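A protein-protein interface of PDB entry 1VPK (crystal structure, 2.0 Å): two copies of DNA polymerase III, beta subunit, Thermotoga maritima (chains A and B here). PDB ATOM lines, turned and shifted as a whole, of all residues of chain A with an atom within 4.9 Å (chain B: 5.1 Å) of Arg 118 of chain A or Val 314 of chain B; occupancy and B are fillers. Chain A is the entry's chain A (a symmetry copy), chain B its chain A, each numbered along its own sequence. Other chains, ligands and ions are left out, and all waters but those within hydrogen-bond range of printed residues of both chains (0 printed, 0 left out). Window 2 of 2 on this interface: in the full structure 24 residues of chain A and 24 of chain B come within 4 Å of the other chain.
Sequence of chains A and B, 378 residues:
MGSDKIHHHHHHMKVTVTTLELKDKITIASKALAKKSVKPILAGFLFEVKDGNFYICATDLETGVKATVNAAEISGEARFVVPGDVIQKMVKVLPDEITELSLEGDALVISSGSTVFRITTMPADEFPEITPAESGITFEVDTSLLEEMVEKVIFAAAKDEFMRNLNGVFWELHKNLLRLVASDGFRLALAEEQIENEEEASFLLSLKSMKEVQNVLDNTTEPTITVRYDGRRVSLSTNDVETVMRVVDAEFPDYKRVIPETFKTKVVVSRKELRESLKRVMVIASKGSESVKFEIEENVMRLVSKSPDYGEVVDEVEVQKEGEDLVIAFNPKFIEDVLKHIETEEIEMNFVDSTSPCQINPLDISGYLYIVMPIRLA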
ATOM      1  N   GLU A 104      23.656 -13.334  -1.858  1.00  0.00           N
ATOM      2  CA  GLU A 104      24.195 -12.526  -0.754  1.00  0.00           C
ATOM      3  C   GLU A 104      23.120 -12.672   0.290  1.00  0.00           C
ATOM      4  O   GLU A 104      21.976 -12.346   0.031  1.00  0.00           O
ATOM      5  CB  GLU A 104      24.417 -11.052  -1.173  1.00  0.00           C
ATOM      6  CG  GLU A 104      24.698 -10.031  -0.008  1.00  0.00           C
ATOM      7  CD  GLU A 104      25.138  -8.622  -0.521  1.00  0.00           C
ATOM      8  OE1 GLU A 104      25.557  -8.506  -1.715  1.00  0.00           O
ATOM      9  OE2 GLU A 104      25.072  -7.649   0.277  1.00  0.00           O
ATOM     10  N   ALA A 107      19.216 -13.620  -0.399  1.00  0.00           N
ATOM     11  CA  ALA A 107      18.774 -12.897  -1.586  1.00  0.00           C
ATOM     12  C   ALA A 107      19.497 -13.417  -2.817  1.00  0.00           C
ATOM     13  O   ALA A 107      20.690 -13.750  -2.734  1.00  0.00           O
ATOM     14  CB  ALA A 107      19.097 -11.410  -1.393  1.00  0.00           C
ATOM     15  N   LEU A 108      18.787 -13.479  -3.948  1.00  0.00           N
ATOM     16  CA  LEU A 108      19.395 -13.573  -5.254  1.00  0.00           C
ATOM     17  C   LEU A 108      19.802 -12.167  -5.692  1.00  0.00           C
ATOM     18  O   LEU A 108      18.967 -11.250  -5.696  1.00  0.00           O
ATOM     19  CB  LEU A 108      18.402 -14.153  -6.287  1.00  0.00           C
ATOM     20  CG  LEU A 108      18.872 -14.248  -7.752  1.00  0.00           C
ATOM     21  CD1 LEU A 108      19.981 -15.309  -7.934  1.00  0.00           C
ATOM     22  CD2 LEU A 108      17.672 -14.593  -8.717  1.00  0.00           C
ATOM     23  N   VAL A 109      21.065 -12.004  -6.057  1.00  0.00           N
ATOM     24  CA  VAL A 109      21.579 -10.740  -6.526  1.00  0.00           C
ATOM     25  C   VAL A 109      21.742 -10.864  -8.037  1.00  0.00           C
ATOM     26  O   VAL A 109      22.392 -11.783  -8.535  1.00  0.00           O
ATOM     27  CB  VAL A 109      22.915 -10.348  -5.887  1.00  0.00           C
ATOM     28  CG1 VAL A 109      23.371  -9.004  -6.455  1.00  0.00           C
ATOM     29  CG2 VAL A 109      22.828 -10.336  -4.387  1.00  0.00           C
ATOM     30  N   SER A 114      24.452  -1.141 -15.185  1.00  0.00           N
ATOM     31  CA  SER A 114      24.130  -0.128 -14.193  1.00  0.00           C
ATOM     32  C   SER A 114      23.213  -0.591 -13.033  1.00  0.00           C
ATOM     33  O   SER A 114      23.106   0.103 -12.023  1.00  0.00           O
ATOM     34  CB  SER A 114      23.385   1.050 -14.911  1.00  0.00           C
ATOM     35  OG  SER A 114      22.110   0.629 -15.493  1.00  0.00           O
ATOM     36  N   THR A 115      22.557  -1.727 -13.196  1.00  0.00           N
ATOM     37  CA  THR A 115      21.456  -2.135 -12.317  1.00  0.00           C
ATOM     38  C   THR A 115      21.839  -3.315 -11.428  1.00  0.00           C
ATOM     39  O   THR A 115      22.516  -4.244 -11.884  1.00  0.00           O
ATOM     40  CB  THR A 115      20.257  -2.545 -13.177  1.00  0.00           C
ATOM     41  OG1 THR A 115      20.139  -1.627 -14.268  1.00  0.00           O
ATOM     42  CG2 THR A 115      18.976  -2.567 -12.366  1.00  0.00           C
ATOM     43  N   VAL A 116      21.356  -3.304 -10.190  1.00  0.00           N
ATOM     44  CA  VAL A 116      21.441  -4.462  -9.315  1.00  0.00           C
ATOM     45  C   VAL A 116      20.063  -4.612  -8.618  1.00  0.00           C
ATOM     46  O   VAL A 116      19.543  -3.678  -8.007  1.00  0.00           O
ATOM     47  CB  VAL A 116      22.607  -4.347  -8.280  1.00  0.00           C
ATOM     48  CG1 VAL A 116      22.701  -5.620  -7.416  1.00  0.00           C
ATOM     49  CG2 VAL A 116      23.911  -4.112  -8.964  1.00  0.00           C
ATOM     50  N   PHE A 117      19.467  -5.774  -8.851  1.00  0.00           N
ATOM     51  CA  PHE A 117      18.270  -6.250  -8.194  1.00  0.00           C
ATOM     52  C   PHE A 117      18.712  -7.248  -7.102  1.00  0.00           C
ATOM     53  O   PHE A 117      19.620  -8.037  -7.324  1.00  0.00           O
ATOM     54  CB  PHE A 117      17.349  -6.946  -9.178  1.00  0.00           C
ATOM     55  CG  PHE A 117      16.558  -6.018 -10.092  1.00  0.00           C
ATOM     56  CD1 PHE A 117      15.318  -5.530  -9.720  1.00  0.00           C
ATOM     57  CD2 PHE A 117      17.042  -5.702 -11.378  1.00  0.00           C
ATOM     58  CE1 PHE A 117      14.572  -4.713 -10.562  1.00  0.00           C
ATOM     59  CE2 PHE A 117      16.292  -4.886 -12.236  1.00  0.00           C
ATOM     60  CZ  PHE A 117      15.057  -4.409 -11.838  1.00  0.00           C
ATOM     61  N   ARG A 118      18.072  -7.172  -5.927  1.00  0.00           N
ATOM     62  CA  ARG A 118      18.268  -8.132  -4.857  1.00  0.00           C
ATOM     63  C   ARG A 118      16.882  -8.678  -4.529  1.00  0.00           C
ATOM     64  O   ARG A 118      16.010  -7.947  -4.125  1.00  0.00           O
ATOM     65  CB  ARG A 118      18.879  -7.465  -3.646  1.00  0.00           C
ATOM     66  CG  ARG A 118      20.298  -7.108  -3.848  1.00  0.00           C
ATOM     67  CD  ARG A 118      20.819  -6.416  -2.597  1.00  0.00           C
ATOM     68  NE  ARG A 118      21.922  -5.488  -2.793  1.00  0.00           N
ATOM     69  CZ  ARG A 118      21.899  -4.395  -3.566  1.00  0.00           C
ATOM     70  NH1 ARG A 118      20.848  -4.074  -4.342  1.00  0.00           N
ATOM     71  NH2 ARG A 118      22.970  -3.620  -3.592  1.00  0.00           N
ATOM     72  N   ILE A 119      16.648  -9.949  -4.866  1.00  0.00           N
ATOM     73  CA  ILE A 119      15.305 -10.528  -4.790  1.00  0.00           C
ATOM     74  C   ILE A 119      15.318 -11.614  -3.711  1.00  0.00           C
ATOM     75  O   ILE A 119      16.124 -12.515  -3.752  1.00  0.00           O
ATOM     76  CB  ILE A 119      14.894 -11.126  -6.170  1.00  0.00           C
ATOM     77  CG1 ILE A 119      15.049 -10.082  -7.298  1.00  0.00           C
ATOM     78  CG2 ILE A 119      13.495 -11.633  -6.152  1.00  0.00           C
ATOM     79  CD1 ILE A 119      14.149  -8.862  -7.154  1.00  0.00           C
ATOM     80  N   THR A 120      14.441 -11.497  -2.725  1.00  0.00           N
ATOM     81  CA  THR A 120      14.317 -12.487  -1.660  1.00  0.00           C
ATOM     82  C   THR A 120      13.912 -13.903  -2.237  1.00  0.00           C
ATOM     83  O   THR A 120      13.075 -14.065  -3.151  1.00  0.00           O
ATOM     84  CB  THR A 120      13.415 -11.840  -0.546  1.00  0.00           C
ATOM     85  OG1 THR A 120      12.508 -10.890  -1.142  1.00  0.00           O
ATOM     86  CG2 THR A 120      14.261 -11.019   0.382  1.00  0.00           C
ATOM     87  N   ARG B 302      22.178   7.593  -8.202  1.00  0.00           N
ATOM     88  CA  ARG B 302      21.635   6.247  -7.991  1.00  0.00           C
ATOM     89  C   ARG B 302      20.154   6.342  -7.682  1.00  0.00           C
ATOM     90  O   ARG B 302      19.742   7.184  -6.874  1.00  0.00           O
ATOM     91  CB  ARG B 302      22.335   5.540  -6.827  1.00  0.00           C
ATOM     92  CG  ARG B 302      23.886   5.423  -6.956  1.00  0.00           C
ATOM     93  CD  ARG B 302      24.507   4.998  -5.622  1.00  0.00           C
ATOM     94  NE  ARG B 302      24.711   3.553  -5.524  1.00  0.00           N
ATOM     95  CZ  ARG B 302      24.519   2.799  -4.429  1.00  0.00           C
ATOM     96  NH1 ARG B 302      24.044   3.312  -3.293  1.00  0.00           N
ATOM     97  NH2 ARG B 302      24.753   1.485  -4.476  1.00  0.00           N
ATOM     98  N   LEU B 303      19.353   5.493  -8.319  1.00  0.00           N
ATOM     99  CA  LEU B 303      17.934   5.417  -8.054  1.00  0.00           C
ATOM    100  C   LEU B 303      17.693   4.133  -7.260  1.00  0.00           C
ATOM    101  O   LEU B 303      18.114   3.062  -7.681  1.00  0.00           O
ATOM    102  CB  LEU B 303      17.071   5.389  -9.337  1.00  0.00           C
ATOM    103  CG  LEU B 303      17.105   6.448 -10.449  1.00  0.00           C
ATOM    104  CD1 LEU B 303      15.765   6.737 -11.041  1.00  0.00           C
ATOM    105  CD2 LEU B 303      17.793   7.695 -10.045  1.00  0.00           C
ATOM    106  N   VAL B 304      17.000   4.237  -6.131  1.00  0.00           N
ATOM    107  CA  VAL B 304      16.861   3.123  -5.235  1.00  0.00           C
ATOM    108  C   VAL B 304      15.401   2.913  -4.903  1.00  0.00           C
ATOM    109  O   VAL B 304      14.707   3.873  -4.516  1.00  0.00           O
ATOM    110  CB  VAL B 304      17.655   3.359  -3.935  1.00  0.00           C
ATOM    111  CG1 VAL B 304      17.415   2.206  -2.906  1.00  0.00           C
ATOM    112  CG2 VAL B 304      19.115   3.524  -4.262  1.00  0.00           C
ATOM    113  N   TYR B 310       9.624  -8.313  -1.431  1.00  0.00           N
ATOM    114  CA  TYR B 310      10.093  -8.789  -2.713  1.00  0.00           C
ATOM    115  C   TYR B 310      11.574  -8.535  -2.981  1.00  0.00           C
ATOM    116  O   TYR B 310      12.255  -9.380  -3.605  1.00  0.00           O
ATOM    117  CB  TYR B 310       9.241  -8.193  -3.814  1.00  0.00           C
ATOM    118  CG  TYR B 310       7.890  -8.824  -3.883  1.00  0.00           C
ATOM    119  CD1 TYR B 310       7.691 -10.000  -4.578  1.00  0.00           C
ATOM    120  CD2 TYR B 310       6.800  -8.232  -3.238  1.00  0.00           C
ATOM    121  CE1 TYR B 310       6.430 -10.582  -4.651  1.00  0.00           C
ATOM    122  CE2 TYR B 310       5.534  -8.792  -3.288  1.00  0.00           C
ATOM    123  CZ  TYR B 310       5.345  -9.961  -4.001  1.00  0.00           C
ATOM    124  OH  TYR B 310       4.082 -10.506  -4.030  1.00  0.00           O
ATOM    125  N   GLY B 311      12.092  -7.404  -2.515  1.00  0.00           N
ATOM    126  CA  GLY B 311      13.483  -7.091  -2.773  1.00  0.00           C
ATOM    127  C   GLY B 311      13.751  -5.622  -2.874  1.00  0.00           C
ATOM    128  O   GLY B 311      12.949  -4.811  -2.355  1.00  0.00           O
ATOM    129  N   GLU B 312      14.903  -5.320  -3.480  1.00  0.00           N
ATOM    130  CA  GLU B 312      15.469  -3.984  -3.663  1.00  0.00           C
ATOM    131  C   GLU B 312      16.028  -3.898  -5.100  1.00  0.00           C
ATOM    132  O   GLU B 312      16.329  -4.919  -5.719  1.00  0.00           O
ATOM    133  CB  GLU B 312      16.630  -3.742  -2.683  1.00  0.00           C
ATOM    134  CG  GLU B 312      16.194  -3.641  -1.203  1.00  0.00           C
ATOM    135  CD  GLU B 312      16.873  -4.677  -0.312  1.00  0.00           C
ATOM    136  OE1 GLU B 312      18.107  -4.877  -0.454  1.00  0.00           O
ATOM    137  OE2 GLU B 312      16.174  -5.299   0.513  1.00  0.00           O
ATOM    138  N   VAL B 313      16.107  -2.681  -5.604  1.00  0.00           N
ATOM    139  CA  VAL B 313      16.797  -2.362  -6.840  1.00  0.00           C
ATOM    140  C   VAL B 313      17.590  -1.083  -6.625  1.00  0.00           C
ATOM    141  O   VAL B 313      17.132  -0.161  -5.958  1.00  0.00           O
ATOM    142  CB  VAL B 313      15.842  -2.193  -8.055  1.00  0.00           C
ATOM    143  CG1 VAL B 313      14.834  -1.077  -7.818  1.00  0.00           C
ATOM    144  CG2 VAL B 313      16.634  -1.969  -9.347  1.00  0.00           C
ATOM    145  N   VAL B 314      18.786  -1.059  -7.191  1.00  0.00           N
ATOM    146  CA  VAL B 314      19.607   0.131  -7.266  1.00  0.00           C
ATOM    147  C   VAL B 314      20.044   0.237  -8.705  1.00  0.00           C
ATOM    148  O   VAL B 314      20.508  -0.744  -9.300  1.00  0.00           O
ATOM    149  CB  VAL B 314      20.847   0.030  -6.363  1.00  0.00           C
ATOM    150  CG1 VAL B 314      21.725   1.292  -6.536  1.00  0.00           C
ATOM    151  CG2 VAL B 314      20.417  -0.208  -4.931  1.00  0.00           C
ATOM    152  N   ASP B 315      19.806   1.391  -9.287  1.00  0.00           N
ATOM    153  CA  ASP B 315      20.244   1.687 -10.644  1.00  0.00           C
ATOM    154  C   ASP B 315      21.082   2.971 -10.665  1.00  0.00           C
ATOM    155  O   ASP B 315      20.656   3.994 -10.187  1.00  0.00           O
ATOM    156  CB  ASP B 315      19.058   1.875 -11.588  1.00  0.00           C
ATOM    157  CG  ASP B 315      19.485   1.825 -13.042  1.00  0.00           C
ATOM    158  OD1 ASP B 315      20.271   0.929 -13.412  1.00  0.00           O
ATOM    159  OD2 ASP B 315      19.090   2.687 -13.820  1.00  0.00           O
ATOM    160  N   GLU B 316      22.244   2.915 -11.282  1.00  0.00           N
ATOM    161  CA  GLU B 316      23.160   4.050 -11.277  1.00  0.00           C
ATOM    162  C   GLU B 316      23.264   4.651 -12.658  1.00  0.00           C
ATOM    163  O   GLU B 316      23.595   3.937 -13.585  1.00  0.00           O
ATOM    164  CB  GLU B 316      24.519   3.565 -10.832  1.00  0.00           C
ATOM    165  CG  GLU B 316      25.571   4.665 -10.769  1.00  0.00           C
ATOM    166  CD  GLU B 316      26.792   4.220  -9.992  1.00  0.00           C
ATOM    167  OE1 GLU B 316      26.688   4.084  -8.764  1.00  0.00           O
ATOM    168  OE2 GLU B 316      27.843   4.007 -10.633  1.00  0.00           O
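O of Tyr 310 of chain B is in hydrogen-bond range of OG1 of Thr 120 of chain A, 2.9 Å away. The backbone NH of Arg 118 of chain A lies within hydrogen-bond range of the backbone carbonyl oxygen of Glu 312 of chain B, 2.9 Å away. The backbone NH of Val 116 of chain A is in hydrogen-bond range of the backbone carbonyl oxygen of Val 314 of chain B. The side-chain carboxylate (OD1) of Asp 315 of chain B lies within hydrogen-bond range of the side-chain hydroxyl (OG) of Ser 114 of chain A (2.8 Å). The side-chain carboxylate (OD1) of Asp 315 of chain B lies within hydrogen-bond range of the side-chain hydroxyl (OG1) of Thr 115 of chain A, at 2.7 Å. The backbone NH (N) of Glu 316 of chain B is in hydrogen-bond range of the backbone carbonyl oxygen (O) of Ser 114 of chain A, at 3.0 Å.
NE of Arg 302 of chain B is in salt-bridge range of OE1 of Glu 316 of chain B (3.8 Å). O of Asp 315 of chain B is in hydrogen-bond range of N of Leu 303 of chain B (2.7 Å). The backbone carbonyl oxygen (O) of Leu 108 of chain A sits at hydrogen-bond distance from the backbone NH (N) of Ile 119 of chain A, 2.8 Å away. The side-chain hydroxyl (OG) of Ser 114 of chain A sits at hydrogen-bond distance from the side-chain hydroxyl (OG1) of Thr 115 of chain A (3.2 Å).
Among the printed residues, pairs that only touch across the chains: Ser 114 of chain A with Val 314 of chain B, Thr 115 of chain A with Val 313 of chain B, Thr 115 of chain A with Val 314 of chain B, Val 116 of chain A with Val 313 of chain B, Phe 117 of chain A with Glu 312 of chain B, Phe 117 of chain A with Val 313 of chain B, Arg 118 of chain A with Gly 311 of chain B, Arg 118 of chain A with Val 314 of chain B, Ile 119 of chain A with Tyr 310 of chain B and Thr 120 of chain A with Gly 311 of chain B.
Leu 108 of chain A touches none of the printed residues of chain B. Of the printed residues of chain B, Thr 115 of chain A touches Val 313, Val 314 and Asp 315. Of the printed residues of chain B, Arg 118 of chain A touches Gly 311 (3.0 Å), Glu 312 (2.9 Å) and Val 314 (3.9 Å). Printed residues of chain B within 4 Å of Thr 120 of chain A: Tyr 310 (2.9 Å) and Gly 311 (3.8 Å). Val 304 of chain B touches none of the printed residues of chain A. Of the printed residues of chain A, Val 313 of chain B touches Thr 115, Val 116 and Phe 117. Of the printed residues of chain A, Val 314 of chain B touches Ser 114, Thr 115, Val 116 and Arg 118. The nearest printed residue of chain B that does not touch Arg 118 of chain A is Tyr 310 of chain B (4.1 Å). The nearest printed residue of chain A that does not touch Val 314 of chain B is Phe 117 of chain A (5.0 Å).
Printed residues of chain B that touch a printed residue of chain A: Tyr 310, Gly 311, Glu 312, Val 313, Val 314, Asp 315 and Glu 316. Hydrophobic or aromatic side chains of chain B within 4 Å of the printed part of chain A: Val 313 and Val 314. Along chain B the printed residues that touch a printed residue of chain A span positions 310 to 316. Along chain A the printed residues that touch a printed residue of chain B span positions 114 to 120. Among the printed residues, 16 pairs touch across the chains. Among the printed residues, no Asp or Glu carboxylate lies within 4 Å of a Lys or Arg side-chain nitrogen of the other chain.
No position is printed for both chains.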
